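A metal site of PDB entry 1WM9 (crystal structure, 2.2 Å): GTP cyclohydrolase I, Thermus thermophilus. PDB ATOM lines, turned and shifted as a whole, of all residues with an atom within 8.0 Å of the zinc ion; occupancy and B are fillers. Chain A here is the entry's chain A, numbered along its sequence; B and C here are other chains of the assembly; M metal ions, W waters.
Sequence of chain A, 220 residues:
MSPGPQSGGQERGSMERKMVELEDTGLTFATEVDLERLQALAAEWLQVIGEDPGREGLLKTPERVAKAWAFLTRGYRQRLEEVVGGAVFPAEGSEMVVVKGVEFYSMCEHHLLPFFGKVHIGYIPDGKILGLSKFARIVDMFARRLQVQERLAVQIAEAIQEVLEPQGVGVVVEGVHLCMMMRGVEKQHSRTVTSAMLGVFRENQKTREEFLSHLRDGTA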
ATOM      1  N   MET A 107      -0.871  19.210 -13.400  1.00  0.00           N
ATOM      2  CA  MET A 107      -2.193  19.618 -12.899  1.00  0.00           C
ATOM      3  C   MET A 107      -2.401  21.075 -13.261  1.00  0.00           C
ATOM      4  O   MET A 107      -1.546  21.916 -12.985  1.00  0.00           O
ATOM      5  CB  MET A 107      -2.240  19.463 -11.382  1.00  0.00           C
ATOM      6  CG  MET A 107      -2.488  18.050 -10.891  1.00  0.00           C
ATOM      7  SD  MET A 107      -4.193  17.547 -11.214  1.00  0.00           S
ATOM      8  CE  MET A 107      -4.329  16.173 -10.117  1.00  0.00           C
ATOM      9  N   CYS A 108      -3.520  21.394 -13.913  1.00  0.00           N
ATOM     10  CA  CYS A 108      -3.754  22.781 -14.261  1.00  0.00           C
ATOM     11  C   CYS A 108      -4.122  23.565 -13.010  1.00  0.00           C
ATOM     12  O   CYS A 108      -4.909  23.103 -12.175  1.00  0.00           O
ATOM     13  CB  CYS A 108      -4.845  22.930 -15.327  1.00  0.00           C
ATOM     14  SG  CYS A 108      -6.503  22.593 -14.753  1.00  0.00           S
ATOM     15  N   GLU A 109      -3.498  24.723 -12.852  1.00  0.00           N
ATOM     16  CA  GLU A 109      -3.750  25.538 -11.677  1.00  0.00           C
ATOM     17  C   GLU A 109      -5.143  26.174 -11.708  1.00  0.00           C
ATOM     18  O   GLU A 109      -5.619  26.658 -10.697  1.00  0.00           O
ATOM     19  CB  GLU A 109      -2.666  26.591 -11.507  1.00  0.00           C
ATOM     20  CG  GLU A 109      -2.643  27.683 -12.567  1.00  0.00           C
ATOM     21  CD  GLU A 109      -1.340  28.479 -12.544  1.00  0.00           C
ATOM     22  OE1 GLU A 109      -0.318  27.950 -12.067  1.00  0.00           O
ATOM     23  OE2 GLU A 109      -1.328  29.638 -13.008  1.00  0.00           O
ATOM     24  N   HIS A 110      -5.805  26.105 -12.861  1.00  0.00           N
ATOM     25  CA  HIS A 110      -7.138  26.684 -12.995  1.00  0.00           C
ATOM     26  C   HIS A 110      -8.303  25.815 -12.520  1.00  0.00           C
ATOM     27  O   HIS A 110      -9.248  26.334 -11.960  1.00  0.00           O
ATOM     28  CB  HIS A 110      -7.374  27.127 -14.441  1.00  0.00           C
ATOM     29  CG  HIS A 110      -6.403  28.151 -14.921  1.00  0.00           C
ATOM     30  ND1 HIS A 110      -6.091  28.319 -16.247  1.00  0.00           N
ATOM     31  CD2 HIS A 110      -5.656  29.061 -14.237  1.00  0.00           C
ATOM     32  CE1 HIS A 110      -5.201  29.282 -16.363  1.00  0.00           C
ATOM     33  NE2 HIS A 110      -4.920  29.751 -15.165  1.00  0.00           N
ATOM     34  N   HIS A 111      -8.225  24.504 -12.739  1.00  0.00           N
ATOM     35  CA  HIS A 111      -9.306  23.603 -12.323  1.00  0.00           C
ATOM     36  C   HIS A 111      -8.840  22.411 -11.486  1.00  0.00           C
ATOM     37  O   HIS A 111      -9.662  21.596 -11.062  1.00  0.00           O
ATOM     38  CB  HIS A 111     -10.041  23.026 -13.543  1.00  0.00           C
ATOM     39  CG  HIS A 111     -10.615  24.057 -14.459  1.00  0.00           C
ATOM     40  ND1 HIS A 111      -9.852  24.696 -15.414  1.00  0.00           N
ATOM     41  CD2 HIS A 111     -11.872  24.530 -14.604  1.00  0.00           C
ATOM     42  CE1 HIS A 111     -10.618  25.529 -16.099  1.00  0.00           C
ATOM     43  NE2 HIS A 111     -11.856  25.440 -15.627  1.00  0.00           N
ATOM     44  N   LEU A 112      -7.536  22.297 -11.275  1.00  0.00           N
ATOM     45  CA  LEU A 112      -6.946  21.177 -10.540  1.00  0.00           C
ATOM     46  C   LEU A 112      -7.266  19.836 -11.199  1.00  0.00           C
ATOM     47  O   LEU A 112      -7.540  18.838 -10.535  1.00  0.00           O
ATOM     48  CB  LEU A 112      -7.364  21.161  -9.059  1.00  0.00           C
ATOM     49  CG  LEU A 112      -7.043  22.368  -8.157  1.00  0.00           C
ATOM     50  CD1 LEU A 112      -7.007  21.904  -6.702  1.00  0.00           C
ATOM     51  CD2 LEU A 112      -5.718  22.996  -8.525  1.00  0.00           C
ATOM     52  N   LEU A 113      -7.261  19.819 -12.531  1.00  0.00           N
ATOM     53  CA  LEU A 113      -7.495  18.600 -13.292  1.00  0.00           C
ATOM     54  C   LEU A 113      -6.231  18.328 -14.090  1.00  0.00           C
ATOM     55  O   LEU A 113      -5.549  19.255 -14.534  1.00  0.00           O
ATOM     56  CB  LEU A 113      -8.715  18.744 -14.216  1.00  0.00           C
ATOM     57  CG  LEU A 113     -10.069  18.743 -13.485  1.00  0.00           C
ATOM     58  CD1 LEU A 113     -11.186  18.997 -14.464  1.00  0.00           C
ATOM     59  CD2 LEU A 113     -10.259  17.408 -12.775  1.00  0.00           C
ATOM     60  N   PRO A 114      -5.899  17.059 -14.317  1.00  0.00           N
ATOM     61  CA  PRO A 114      -4.679  16.761 -15.065  1.00  0.00           C
ATOM     62  C   PRO A 114      -4.621  17.175 -16.529  1.00  0.00           C
ATOM     63  O   PRO A 114      -5.634  17.257 -17.225  1.00  0.00           O
ATOM     64  CB  PRO A 114      -4.575  15.231 -14.948  1.00  0.00           C
ATOM     65  CG  PRO A 114      -5.394  14.886 -13.727  1.00  0.00           C
ATOM     66  CD  PRO A 114      -6.571  15.817 -13.909  1.00  0.00           C
ATOM     67  N   PHE A 115      -3.416  17.523 -16.942  1.00  0.00           N
ATOM     68  CA  PHE A 115      -3.132  17.808 -18.329  1.00  0.00           C
ATOM     69  C   PHE A 115      -1.803  17.078 -18.535  1.00  0.00           C
ATOM     70  O   PHE A 115      -0.936  17.073 -17.643  1.00  0.00           O
ATOM     71  CB  PHE A 115      -3.129  19.315 -18.674  1.00  0.00           C
ATOM     72  CG  PHE A 115      -1.921  20.075 -18.222  1.00  0.00           C
ATOM     73  CD1 PHE A 115      -1.936  20.751 -17.005  1.00  0.00           C
ATOM     74  CD2 PHE A 115      -0.837  20.260 -19.070  1.00  0.00           C
ATOM     75  CE1 PHE A 115      -0.887  21.610 -16.650  1.00  0.00           C
ATOM     76  CE2 PHE A 115       0.214  21.112 -18.726  1.00  0.00           C
ATOM     77  CZ  PHE A 115       0.183  21.787 -17.514  1.00  0.00           C
ATOM     78  N   GLN A 147       0.256  23.913 -12.677  1.00  0.00           N
ATOM     79  CA  GLN A 147       0.815  24.632 -13.809  1.00  0.00           C
ATOM     80  C   GLN A 147      -0.166  25.093 -14.881  1.00  0.00           C
ATOM     81  O   GLN A 147      -1.363  24.843 -14.808  1.00  0.00           O
ATOM     82  CB  GLN A 147       1.818  23.693 -14.511  1.00  0.00           C
ATOM     83  CG  GLN A 147       3.188  23.560 -13.844  1.00  0.00           C
ATOM     84  CD  GLN A 147       4.096  24.714 -14.193  1.00  0.00           C
ATOM     85  OE1 GLN A 147       3.658  25.710 -14.772  1.00  0.00           O
ATOM     86  NE2 GLN A 147       5.378  24.595 -13.836  1.00  0.00           N
ATOM     87  N   VAL A 148       0.380  25.860 -15.820  1.00  0.00           N
ATOM     88  CA  VAL A 148      -0.308  26.311 -17.040  1.00  0.00           C
ATOM     89  C   VAL A 148       0.781  25.905 -18.043  1.00  0.00           C
ATOM     90  O   VAL A 148       1.979  26.113 -17.794  1.00  0.00           O
ATOM     91  CB  VAL A 148      -0.628  27.837 -17.111  1.00  0.00           C
ATOM     92  CG1 VAL A 148      -1.704  28.181 -16.087  1.00  0.00           C
ATOM     93  CG2 VAL A 148       0.593  28.687 -16.903  1.00  0.00           C
ATOM     94  N   HIS A 177      -5.694  18.421 -22.347  1.00  0.00           N
ATOM     95  CA  HIS A 177      -6.176  18.924 -21.058  1.00  0.00           C
ATOM     96  C   HIS A 177      -7.544  18.382 -20.690  1.00  0.00           C
ATOM     97  O   HIS A 177      -8.530  18.626 -21.385  1.00  0.00           O
ATOM     98  CB  HIS A 177      -6.222  20.459 -21.100  1.00  0.00           C
ATOM     99  CG  HIS A 177      -4.900  21.092 -21.392  1.00  0.00           C
ATOM    100  ND1 HIS A 177      -4.336  22.046 -20.572  1.00  0.00           N
ATOM    101  CD2 HIS A 177      -4.011  20.891 -22.401  1.00  0.00           C
ATOM    102  CE1 HIS A 177      -3.155  22.390 -21.050  1.00  0.00           C
ATOM    103  NE2 HIS A 177      -2.936  21.708 -22.159  1.00  0.00           N
ATOM    104  N   LEU A 178      -7.613  17.647 -19.574  1.00  0.00           N
ATOM    105  CA  LEU A 178      -8.875  17.068 -19.115  1.00  0.00           C
ATOM    106  C   LEU A 178      -9.926  18.095 -18.699  1.00  0.00           C
ATOM    107  O   LEU A 178     -11.130  17.815 -18.749  1.00  0.00           O
ATOM    108  CB  LEU A 178      -8.641  16.058 -17.993  1.00  0.00           C
ATOM    109  CG  LEU A 178      -7.996  14.735 -18.393  1.00  0.00           C
ATOM    110  CD1 LEU A 178      -7.988  13.814 -17.196  1.00  0.00           C
ATOM    111  CD2 LEU A 178      -8.754  14.092 -19.548  1.00  0.00           C
ATOM    112  N   CYS A 179      -9.494  19.284 -18.283  1.00  0.00           N
ATOM    113  CA  CYS A 179     -10.443  20.316 -17.894  1.00  0.00           C
ATOM    114  C   CYS A 179     -11.204  20.815 -19.133  1.00  0.00           C
ATOM    115  O   CYS A 179     -12.184  21.560 -19.022  1.00  0.00           O
ATOM    116  CB  CYS A 179      -9.720  21.475 -17.186  1.00  0.00           C
ATOM    117  SG  CYS A 179      -8.534  22.385 -18.215  1.00  0.00           S
ATOM    118  N   MET A 180     -10.752  20.377 -20.299  1.00  0.00           N
ATOM    119  CA  MET A 180     -11.351  20.746 -21.577  1.00  0.00           C
ATOM    120  C   MET A 180     -12.094  19.564 -22.212  1.00  0.00           C
ATOM    121  O   MET A 180     -12.934  19.726 -23.082  1.00  0.00           O
ATOM    122  CB  MET A 180     -10.254  21.250 -22.536  1.00  0.00           C
ATOM    123  CG  MET A 180     -10.730  21.676 -23.916  1.00  0.00           C
ATOM    124  SD  MET A 180      -9.434  22.511 -24.904  1.00  0.00           S
ATOM    125  CE  MET A 180      -8.312  22.991 -23.646  1.00  0.00           C
ATOM    126  N   ARG A 183     -14.964  18.026 -18.877  1.00  0.00           N
ATOM    127  CA  ARG A 183     -15.985  18.982 -18.457  1.00  0.00           C
ATOM    128  C   ARG A 183     -16.052  20.212 -19.355  1.00  0.00           C
ATOM    129  O   ARG A 183     -15.326  20.302 -20.356  1.00  0.00           O
ATOM    130  CB  ARG A 183     -15.686  19.445 -17.019  1.00  0.00           C
ATOM    131  CG  ARG A 183     -14.262  19.961 -16.830  1.00  0.00           C
ATOM    132  CD  ARG A 183     -14.140  20.910 -15.648  1.00  0.00           C
ATOM    133  NE  ARG A 183     -15.027  22.070 -15.789  1.00  0.00           N
ATOM    134  CZ  ARG A 183     -14.777  23.126 -16.545  1.00  0.00           C
ATOM    135  NH1 ARG A 183     -13.650  23.215 -17.243  1.00  0.00           N
ATOM    136  NH2 ARG A 183     -15.687  24.089 -16.654  1.00  0.00           N
ATOM    137  N   GLY B 131      -7.521  31.368 -21.374  1.00  0.00           N
ATOM    138  CA  GLY B 131      -7.739  30.043 -20.846  1.00  0.00           C
ATOM    139  C   GLY B 131      -8.044  29.183 -22.064  1.00  0.00           C
ATOM    140  O   GLY B 131      -8.884  29.554 -22.884  1.00  0.00           O
ATOM    141  N   LEU B 132      -7.335  28.075 -22.214  1.00  0.00           N
ATOM    142  CA  LEU B 132      -7.497  27.191 -23.364  1.00  0.00           C
ATOM    143  C   LEU B 132      -8.925  26.864 -23.809  1.00  0.00           C
ATOM    144  O   LEU B 132      -9.257  26.984 -24.997  1.00  0.00           O
ATOM    145  CB  LEU B 132      -6.703  25.901 -23.159  1.00  0.00           C
ATOM    146  CG  LEU B 132      -5.195  26.088 -22.904  1.00  0.00           C
ATOM    147  CD1 LEU B 132      -4.525  24.737 -22.853  1.00  0.00           C
ATOM    148  CD2 LEU B 132      -4.556  26.937 -23.988  1.00  0.00           C
ATOM    149  N   SER B 133      -9.781  26.487 -22.860  1.00  0.00           N
ATOM    150  CA  SER B 133     -11.166  26.134 -23.159  1.00  0.00           C
ATOM    151  C   SER B 133     -11.995  27.286 -23.747  1.00  0.00           C
ATOM    152  O   SER B 133     -13.027  27.045 -24.393  1.00  0.00           O
ATOM    153  CB  SER B 133     -11.848  25.615 -21.901  1.00  0.00           C
ATOM    154  OG  SER B 133     -11.820  26.589 -20.879  1.00  0.00           O
ATOM    155  N   ARG C  64     -13.747  27.497  -9.368  1.00  0.00           N
ATOM    156  CA  ARG C  64     -13.742  26.653 -10.560  1.00  0.00           C
ATOM    157  C   ARG C  64     -13.751  25.183 -10.172  1.00  0.00           C
ATOM    158  O   ARG C  64     -14.490  24.393 -10.760  1.00  0.00           O
ATOM    159  CB  ARG C  64     -12.549  26.997 -11.468  1.00  0.00           C
ATOM    160  CG  ARG C  64     -12.742  28.299 -12.241  1.00  0.00           C
ATOM    161  CD  ARG C  64     -11.632  28.588 -13.233  1.00  0.00           C
ATOM    162  NE  ARG C  64     -10.363  28.922 -12.582  1.00  0.00           N
ATOM    163  CZ  ARG C  64      -9.733  30.090 -12.704  1.00  0.00           C
ATOM    164  NH1 ARG C  64     -10.256  31.054 -13.453  1.00  0.00           N
ATOM    165  NH2 ARG C  64      -8.577  30.287 -12.088  1.00  0.00           N
HETATM  166 ZN    ZN M   1      -7.870  23.826 -16.579  1.00  0.00          ZN
HETATM  167  O   HOH W   1      -5.643  25.471 -18.274  1.00  0.00           O
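A ring nitrogen (NE2) of His 111 lies within hydrogen-bond range of the guanidinium group (NH1) of Arg 183, at 3.3 Å.
The backbone carbonyl oxygen (O) of Cys 179 lies within hydrogen-bond range of the guanidinium group (NH1) of Arg 183 (2.8 Å).
The backbone carbonyl oxygen of His 110 sits at hydrogen-bond distance from the guanidinium group of Arg 64 of chain C (2.9 Å).
N of Cys 108 is in hydrogen-bond range of O of Leu 113, at 3.0 Å.
The side-chain sulfur of Cys 108 lies close to the backbone NH of Leu 112 (3.6 Å).
Residues that only touch the zinc ion: His 110.
Four residues have an atom within 4 Å of the zinc ion: Cys 108, His 110, His 111 and Cys 179.
The zinc ion is bound by SG of Cys 179 (2.3 Å), ND1 of His 111 (2.5 Å) and SG of Cys 108 (2.6 Å).
The zinc ion has three donor atoms within binding distance.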
